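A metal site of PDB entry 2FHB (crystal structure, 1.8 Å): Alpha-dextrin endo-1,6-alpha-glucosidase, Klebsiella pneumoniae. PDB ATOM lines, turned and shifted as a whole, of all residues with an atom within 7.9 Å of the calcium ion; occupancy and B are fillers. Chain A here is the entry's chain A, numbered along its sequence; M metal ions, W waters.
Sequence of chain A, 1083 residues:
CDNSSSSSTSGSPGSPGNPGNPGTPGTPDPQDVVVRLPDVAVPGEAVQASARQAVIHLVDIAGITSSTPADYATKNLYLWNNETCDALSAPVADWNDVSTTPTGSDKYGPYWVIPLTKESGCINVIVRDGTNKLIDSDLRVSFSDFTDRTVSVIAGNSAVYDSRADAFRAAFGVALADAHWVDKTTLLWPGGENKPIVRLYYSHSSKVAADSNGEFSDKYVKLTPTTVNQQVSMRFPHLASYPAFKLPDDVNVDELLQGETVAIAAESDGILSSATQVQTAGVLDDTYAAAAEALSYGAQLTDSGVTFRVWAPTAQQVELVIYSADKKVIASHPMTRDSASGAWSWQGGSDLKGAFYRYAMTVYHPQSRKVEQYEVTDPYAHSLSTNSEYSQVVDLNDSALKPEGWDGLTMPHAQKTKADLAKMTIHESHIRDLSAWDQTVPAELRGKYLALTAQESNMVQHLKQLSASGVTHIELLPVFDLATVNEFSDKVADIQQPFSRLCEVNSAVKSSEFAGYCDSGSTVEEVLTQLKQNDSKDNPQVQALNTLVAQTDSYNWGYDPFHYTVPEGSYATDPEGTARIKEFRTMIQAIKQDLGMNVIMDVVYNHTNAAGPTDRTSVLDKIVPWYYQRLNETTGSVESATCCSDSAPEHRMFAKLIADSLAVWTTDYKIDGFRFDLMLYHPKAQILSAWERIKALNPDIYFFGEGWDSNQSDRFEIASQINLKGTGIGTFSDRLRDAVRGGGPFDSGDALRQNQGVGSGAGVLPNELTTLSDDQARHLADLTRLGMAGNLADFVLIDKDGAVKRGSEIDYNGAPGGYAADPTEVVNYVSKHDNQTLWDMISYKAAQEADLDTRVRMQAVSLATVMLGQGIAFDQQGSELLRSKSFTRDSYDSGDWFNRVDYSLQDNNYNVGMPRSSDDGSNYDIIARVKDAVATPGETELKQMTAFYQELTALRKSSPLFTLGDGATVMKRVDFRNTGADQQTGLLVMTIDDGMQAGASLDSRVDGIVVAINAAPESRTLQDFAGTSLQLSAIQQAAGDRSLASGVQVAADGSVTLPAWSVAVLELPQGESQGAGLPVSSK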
ATOM      1  N   LEU A 384      -0.609   7.810 -13.027  1.00  0.00           N
ATOM      2  CA  LEU A 384      -0.873   7.251 -14.353  1.00  0.00           C
ATOM      3  C   LEU A 384      -0.707   5.736 -14.410  1.00  0.00           C
ATOM      4  O   LEU A 384      -0.085   5.122 -13.533  1.00  0.00           O
ATOM      5  CB  LEU A 384       0.100   7.858 -15.375  1.00  0.00           C
ATOM      6  CG  LEU A 384       0.125   9.379 -15.592  1.00  0.00           C
ATOM      7  CD1 LEU A 384       1.437   9.796 -16.273  1.00  0.00           C
ATOM      8  CD2 LEU A 384      -1.078   9.769 -16.441  1.00  0.00           C
ATOM      9  N   SER A 385      -1.260   5.142 -15.471  1.00  0.00           N
ATOM     10  CA  SER A 385      -1.118   3.712 -15.720  1.00  0.00           C
ATOM     11  C   SER A 385       0.158   3.585 -16.556  1.00  0.00           C
ATOM     12  O   SER A 385       0.797   4.599 -16.876  1.00  0.00           O
ATOM     13  CB  SER A 385      -2.307   3.173 -16.529  1.00  0.00           C
ATOM     14  OG  SER A 385      -2.352   3.730 -17.833  1.00  0.00           O
ATOM     15  N   THR A 386       0.534   2.359 -16.908  1.00  0.00           N
ATOM     16  CA  THR A 386       1.747   2.147 -17.699  1.00  0.00           C
ATOM     17  C   THR A 386       1.759   2.918 -19.022  1.00  0.00           C
ATOM     18  O   THR A 386       0.786   2.911 -19.773  1.00  0.00           O
ATOM     19  CB  THR A 386       1.958   0.646 -17.999  1.00  0.00           C
ATOM     20  OG1 THR A 386       2.022  -0.077 -16.756  1.00  0.00           O
ATOM     21  CG2 THR A 386       3.261   0.432 -18.761  1.00  0.00           C
ATOM     22  N   ASN A 387       2.890   3.573 -19.295  1.00  0.00           N
ATOM     23  CA  ASN A 387       3.091   4.370 -20.500  1.00  0.00           C
ATOM     24  C   ASN A 387       2.130   5.553 -20.619  1.00  0.00           C
ATOM     25  O   ASN A 387       1.914   6.084 -21.721  1.00  0.00           O
ATOM     26  CB  ASN A 387       2.987   3.485 -21.757  1.00  0.00           C
ATOM     27  CG  ASN A 387       3.934   3.929 -22.865  1.00  0.00           C
ATOM     28  OD1 ASN A 387       3.659   3.735 -24.056  1.00  0.00           O
ATOM     29  ND2 ASN A 387       5.067   4.520 -22.491  1.00  0.00           N
ATOM     30  N   SER A 388       1.554   5.973 -19.495  1.00  0.00           N
ATOM     31  CA  SER A 388       0.658   7.126 -19.446  1.00  0.00           C
ATOM     32  C   SER A 388      -0.638   7.051 -20.257  1.00  0.00           C
ATOM     33  O   SER A 388      -1.175   8.073 -20.670  1.00  0.00           O
ATOM     34  CB  SER A 388       1.424   8.393 -19.881  1.00  0.00           C
ATOM     35  OG  SER A 388       2.749   8.380 -19.378  1.00  0.00           O
ATOM     36  N   PHE A 480      10.039  13.843 -14.326  1.00  0.00           N
ATOM     37  CA  PHE A 480       8.589  14.018 -14.439  1.00  0.00           C
ATOM     38  C   PHE A 480       8.263  13.053 -15.583  1.00  0.00           C
ATOM     39  O   PHE A 480       9.175  12.416 -16.125  1.00  0.00           O
ATOM     40  CB  PHE A 480       8.225  15.469 -14.820  1.00  0.00           C
ATOM     41  CG  PHE A 480       9.020  16.011 -15.973  1.00  0.00           C
ATOM     42  CD1 PHE A 480       8.643  15.736 -17.283  1.00  0.00           C
ATOM     43  CD2 PHE A 480      10.170  16.748 -15.741  1.00  0.00           C
ATOM     44  CE1 PHE A 480       9.412  16.201 -18.347  1.00  0.00           C
ATOM     45  CE2 PHE A 480      10.958  17.218 -16.795  1.00  0.00           C
ATOM     46  CZ  PHE A 480      10.572  16.938 -18.105  1.00  0.00           C
ATOM     47  N   ASP A 481       6.991  12.923 -15.966  1.00  0.00           N
ATOM     48  CA  ASP A 481       6.631  11.981 -17.034  1.00  0.00           C
ATOM     49  C   ASP A 481       7.034  12.355 -18.452  1.00  0.00           C
ATOM     50  O   ASP A 481       6.401  13.185 -19.092  1.00  0.00           O
ATOM     51  CB  ASP A 481       5.123  11.690 -17.012  1.00  0.00           C
ATOM     52  CG  ASP A 481       4.708  10.647 -18.021  1.00  0.00           C
ATOM     53  OD1 ASP A 481       5.480   9.670 -18.228  1.00  0.00           O
ATOM     54  OD2 ASP A 481       3.608  10.769 -18.597  1.00  0.00           O
ATOM     55  N   LEU A 482       8.107  11.728 -18.937  1.00  0.00           N
ATOM     56  CA  LEU A 482       8.610  11.969 -20.284  1.00  0.00           C
ATOM     57  C   LEU A 482       7.918  10.998 -21.238  1.00  0.00           C
ATOM     58  O   LEU A 482       7.361   9.977 -20.809  1.00  0.00           O
ATOM     59  CB  LEU A 482      10.134  11.799 -20.333  1.00  0.00           C
ATOM     60  CG  LEU A 482      10.729  10.483 -19.815  1.00  0.00           C
ATOM     61  CD1 LEU A 482      11.380   9.728 -20.976  1.00  0.00           C
ATOM     62  CD2 LEU A 482      11.755  10.776 -18.730  1.00  0.00           C
ATOM     63  N   ALA A 483       7.965  11.284 -22.535  1.00  0.00           N
ATOM     64  CA  ALA A 483       7.286  10.439 -23.502  1.00  0.00           C
ATOM     65  C   ALA A 483       8.147   9.533 -24.380  1.00  0.00           C
ATOM     66  O   ALA A 483       7.625   8.567 -24.957  1.00  0.00           O
ATOM     67  CB  ALA A 483       6.422  11.309 -24.402  1.00  0.00           C
ATOM     68  N   THR A 484       9.444   9.801 -24.446  1.00  0.00           N
ATOM     69  CA  THR A 484      10.351   9.059 -25.323  1.00  0.00           C
ATOM     70  C   THR A 484      10.969   7.720 -24.891  1.00  0.00           C
ATOM     71  O   THR A 484      11.980   7.284 -25.456  1.00  0.00           O
ATOM     72  CB  THR A 484      11.467  10.015 -25.797  1.00  0.00           C
ATOM     73  OG1 THR A 484      12.007  10.721 -24.673  1.00  0.00           O
ATOM     74  CG2 THR A 484      10.895  11.037 -26.771  1.00  0.00           C
ATOM     75  N   VAL A 485      10.368   7.072 -23.902  1.00  0.00           N
ATOM     76  CA  VAL A 485      10.804   5.749 -23.463  1.00  0.00           C
ATOM     77  C   VAL A 485       9.522   4.961 -23.236  1.00  0.00           C
ATOM     78  O   VAL A 485       8.607   5.422 -22.536  1.00  0.00           O
ATOM     79  CB  VAL A 485      11.626   5.800 -22.150  1.00  0.00           C
ATOM     80  CG1 VAL A 485      11.804   4.379 -21.603  1.00  0.00           C
ATOM     81  CG2 VAL A 485      13.013   6.403 -22.406  1.00  0.00           C
ATOM     82  N   ASN A 486       9.419   3.786 -23.854  1.00  0.00           N
ATOM     83  CA  ASN A 486       8.222   2.968 -23.706  1.00  0.00           C
ATOM     84  C   ASN A 486       8.244   2.331 -22.326  1.00  0.00           C
ATOM     85  O   ASN A 486       9.198   1.648 -21.964  1.00  0.00           O
ATOM     86  CB  ASN A 486       8.182   1.888 -24.793  1.00  0.00           C
ATOM     87  CG  ASN A 486       6.801   1.257 -24.935  1.00  0.00           C
ATOM     88  OD1 ASN A 486       6.182   0.870 -23.948  1.00  0.00           O
ATOM     89  ND2 ASN A 486       6.320   1.156 -26.176  1.00  0.00           N
ATOM     90  N   GLU A 487       7.188   2.549 -21.538  1.00  0.00           N
ATOM     91  CA  GLU A 487       7.136   1.991 -20.183  1.00  0.00           C
ATOM     92  C   GLU A 487       6.675   0.529 -20.142  1.00  0.00           C
ATOM     93  O   GLU A 487       6.665  -0.086 -19.069  1.00  0.00           O
ATOM     94  CB  GLU A 487       6.271   2.878 -19.279  1.00  0.00           C
ATOM     95  CG  GLU A 487       6.685   4.366 -19.343  1.00  0.00           C
ATOM     96  CD  GLU A 487       6.019   5.232 -18.280  1.00  0.00           C
ATOM     97  OE1 GLU A 487       5.009   4.810 -17.692  1.00  0.00           O
ATOM     98  OE2 GLU A 487       6.519   6.355 -18.040  1.00  0.00           O
ATOM     99  N   ASP A 560      11.176  15.716 -22.964  1.00  0.00           N
ATOM    100  CA  ASP A 560      10.000  15.452 -23.809  1.00  0.00           C
ATOM    101  C   ASP A 560       8.785  15.265 -22.891  1.00  0.00           C
ATOM    102  O   ASP A 560       8.345  14.137 -22.659  1.00  0.00           O
ATOM    103  CB  ASP A 560      10.263  14.181 -24.628  1.00  0.00           C
ATOM    104  CG  ASP A 560      11.568  14.236 -25.404  1.00  0.00           C
ATOM    105  OD1 ASP A 560      12.475  13.428 -25.125  1.00  0.00           O
ATOM    106  OD2 ASP A 560      11.687  15.112 -26.296  1.00  0.00           O
ATOM    107  N   PHE A 562       5.285  14.716 -21.201  1.00  0.00           N
ATOM    108  CA  PHE A 562       4.035  14.029 -21.502  1.00  0.00           C
ATOM    109  C   PHE A 562       3.031  14.553 -20.451  1.00  0.00           C
ATOM    110  O   PHE A 562       1.959  15.031 -20.800  1.00  0.00           O
ATOM    111  CB  PHE A 562       4.222  12.506 -21.406  1.00  0.00           C
ATOM    112  CG  PHE A 562       3.172  11.695 -22.125  1.00  0.00           C
ATOM    113  CD1 PHE A 562       3.401  10.347 -22.414  1.00  0.00           C
ATOM    114  CD2 PHE A 562       1.963  12.264 -22.515  1.00  0.00           C
ATOM    115  CE1 PHE A 562       2.450   9.573 -23.073  1.00  0.00           C
ATOM    116  CE2 PHE A 562       0.989  11.492 -23.180  1.00  0.00           C
ATOM    117  CZ  PHE A 562       1.237  10.149 -23.458  1.00  0.00           C
ATOM    118  N   HIS A 563       3.420  14.461 -19.172  1.00  0.00           N
ATOM    119  CA  HIS A 563       2.611  14.972 -18.059  1.00  0.00           C
ATOM    120  C   HIS A 563       3.584  15.679 -17.095  1.00  0.00           C
ATOM    121  O   HIS A 563       4.590  15.097 -16.674  1.00  0.00           O
ATOM    122  CB  HIS A 563       1.876  13.834 -17.339  1.00  0.00           C
ATOM    123  CG  HIS A 563       0.898  13.113 -18.206  1.00  0.00           C
ATOM    124  ND1 HIS A 563      -0.414  13.501 -18.342  1.00  0.00           N
ATOM    125  CD2 HIS A 563       1.063  12.039 -19.027  1.00  0.00           C
ATOM    126  CE1 HIS A 563      -1.020  12.712 -19.222  1.00  0.00           C
ATOM    127  NE2 HIS A 563      -0.143  11.822 -19.643  1.00  0.00           N
ATOM    128  N   VAL A 566       3.604  14.230 -12.692  1.00  0.00           N
ATOM    129  CA  VAL A 566       3.591  12.812 -12.374  1.00  0.00           C
ATOM    130  C   VAL A 566       5.028  12.316 -12.587  1.00  0.00           C
ATOM    131  O   VAL A 566       5.683  12.715 -13.539  1.00  0.00           O
ATOM    132  CB  VAL A 566       2.670  12.005 -13.322  1.00  0.00           C
ATOM    133  CG1 VAL A 566       2.597  10.541 -12.869  1.00  0.00           C
ATOM    134  CG2 VAL A 566       1.282  12.617 -13.378  1.00  0.00           C
ATOM    135  N   PRO A 567       5.538  11.463 -11.682  1.00  0.00           N
ATOM    136  CA  PRO A 567       6.911  10.975 -11.867  1.00  0.00           C
ATOM    137  C   PRO A 567       7.012  10.065 -13.095  1.00  0.00           C
ATOM    138  O   PRO A 567       6.009   9.478 -13.513  1.00  0.00           O
ATOM    139  CB  PRO A 567       7.198  10.210 -10.572  1.00  0.00           C
ATOM    140  CG  PRO A 567       6.323  10.926  -9.565  1.00  0.00           C
ATOM    141  CD  PRO A 567       5.046  11.121 -10.335  1.00  0.00           C
ATOM    142  N   GLU A 568       8.208   9.965 -13.681  1.00  0.00           N
ATOM    143  CA  GLU A 568       8.434   9.105 -14.845  1.00  0.00           C
ATOM    144  C   GLU A 568       8.203   7.648 -14.451  1.00  0.00           C
ATOM    145  O   GLU A 568       8.614   7.227 -13.371  1.00  0.00           O
ATOM    146  CB  GLU A 568       9.868   9.288 -15.365  1.00  0.00           C
ATOM    147  CG  GLU A 568      10.376   8.148 -16.250  1.00  0.00           C
ATOM    148  CD  GLU A 568       9.568   7.959 -17.526  1.00  0.00           C
ATOM    149  OE1 GLU A 568       9.864   6.984 -18.269  1.00  0.00           O
ATOM    150  OE2 GLU A 568       8.646   8.753 -17.798  1.00  0.00           O
ATOM    151  N   GLY A 569       7.558   6.889 -15.331  1.00  0.00           N
ATOM    152  CA  GLY A 569       7.261   5.487 -15.022  1.00  0.00           C
ATOM    153  C   GLY A 569       8.362   4.459 -15.247  1.00  0.00           C
ATOM    154  O   GLY A 569       8.434   3.479 -14.506  1.00  0.00           O
ATOM    155  N   SER A 570       9.215   4.675 -16.245  1.00  0.00           N
ATOM    156  CA  SER A 570      10.283   3.720 -16.528  1.00  0.00           C
ATOM    157  C   SER A 570      11.364   3.648 -15.458  1.00  0.00           C
ATOM    158  O   SER A 570      12.121   2.684 -15.412  1.00  0.00           O
ATOM    159  CB  SER A 570      10.923   4.027 -17.887  1.00  0.00           C
ATOM    160  OG  SER A 570      11.748   5.178 -17.807  1.00  0.00           O
ATOM    161  N   TYR A 571      11.447   4.658 -14.591  1.00  0.00           N
ATOM    162  CA  TYR A 571      12.442   4.658 -13.524  1.00  0.00           C
ATOM    163  C   TYR A 571      11.921   3.950 -12.269  1.00  0.00           C
ATOM    164  O   TYR A 571      12.630   3.840 -11.268  1.00  0.00           O
ATOM    165  CB  TYR A 571      12.873   6.090 -13.182  1.00  0.00           C
ATOM    166  CG  TYR A 571      13.555   6.833 -14.319  1.00  0.00           C
ATOM    167  CD1 TYR A 571      14.399   6.170 -15.210  1.00  0.00           C
ATOM    168  CD2 TYR A 571      13.388   8.213 -14.486  1.00  0.00           C
ATOM    169  CE1 TYR A 571      15.065   6.852 -16.228  1.00  0.00           C
ATOM    170  CE2 TYR A 571      14.048   8.907 -15.508  1.00  0.00           C
ATOM    171  CZ  TYR A 571      14.884   8.212 -16.380  1.00  0.00           C
ATOM    172  OH  TYR A 571      15.553   8.889 -17.390  1.00  0.00           O
ATOM    173  N   ARG A 580       5.072   4.120  -8.423  1.00  0.00           N
ATOM    174  CA  ARG A 580       6.158   5.049  -8.721  1.00  0.00           C
ATOM    175  C   ARG A 580       6.238   6.232  -7.770  1.00  0.00           C
ATOM    176  O   ARG A 580       7.316   6.792  -7.565  1.00  0.00           O
ATOM    177  CB  ARG A 580       6.042   5.554 -10.157  1.00  0.00           C
ATOM    178  CG  ARG A 580       4.995   6.636 -10.328  1.00  0.00           C
ATOM    179  CD  ARG A 580       4.892   7.083 -11.786  1.00  0.00           C
ATOM    180  NE  ARG A 580       4.208   6.094 -12.624  1.00  0.00           N
ATOM    181  CZ  ARG A 580       3.869   6.300 -13.883  1.00  0.00           C
ATOM    182  NH1 ARG A 580       4.143   7.469 -14.456  1.00  0.00           N
ATOM    183  NH2 ARG A 580       3.235   5.356 -14.578  1.00  0.00           N
ATOM    184  N   ARG A 616      -0.339  10.648 -30.114  1.00  0.00           N
ATOM    185  CA  ARG A 616      -0.542   9.944 -28.846  1.00  0.00           C
ATOM    186  C   ARG A 616      -0.171  10.791 -27.625  1.00  0.00           C
ATOM    187  O   ARG A 616      -0.836  10.725 -26.591  1.00  0.00           O
ATOM    188  CB  ARG A 616       0.319   8.675 -28.837  1.00  0.00           C
ATOM    189  CG  ARG A 616       0.409   7.946 -27.498  1.00  0.00           C
ATOM    190  CD  ARG A 616       1.303   6.722 -27.586  1.00  0.00           C
ATOM    191  NE  ARG A 616       2.717   7.060 -27.808  1.00  0.00           N
ATOM    192  CZ  ARG A 616       3.611   7.224 -26.839  1.00  0.00           C
ATOM    193  NH1 ARG A 616       3.266   7.067 -25.567  1.00  0.00           N
ATOM    194  NH2 ARG A 616       4.864   7.539 -27.138  1.00  0.00           N
HETATM  195 CA    CA M   1       6.813   8.300 -19.368  1.00  0.00          CA
HETATM  196  O   HOH W   1       5.063   7.574 -20.756  1.00  0.00           O
HETATM  197  O   HOH W   2       8.389   7.152 -20.672  1.00  0.00           O
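The calcium ion is bound by the side-chain carboxylate of Asp 481, the backbone carbonyl oxygen of Leu 482, water W2, water W1, the side-chain carboxylate of Glu 487 and the side-chain carboxylate of Glu 568.
Four residues have an atom within 4 Å of the calcium ion: Asp 481, Leu 482, Glu 487 and Glu 568. The nearest printed residue that does not touch the calcium ion is Ser 388 (4.1 Å).
The side-chain hydroxyl (OG) of Ser 388 lies within hydrogen-bond range of the side-chain carboxylate (OD2) of Asp 481, at 2.7 Å. The backbone carbonyl oxygen of Asp 481 lies within hydrogen-bond range of the backbone NH of Phe 562. The backbone NH (N) of His 563 sits at hydrogen-bond distance from the backbone carbonyl oxygen (O) of Asp 481 (3.2 Å). N of Asp 481 is in hydrogen-bond range of O of Val 566 (2.8 Å). The backbone NH (N) of Gly 569 lies close to the side-chain carboxylate (OE2) of Glu 487 (3.0 Å). The side-chain carboxylate (OE1) of Glu 487 is in hydrogen-bond range of the backbone NH (N) of Asn 387, 2.9 Å away. NH2 of Arg 580 is in salt-bridge range of OE1 of Glu 487, 3.6 Å away. OE1 of Glu 568 lies within hydrogen-bond range of OG of Ser 570.
Water W2 bridges O of Val 485 (2.6 Å) and OE1 of Glu 568 (2.8 Å).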
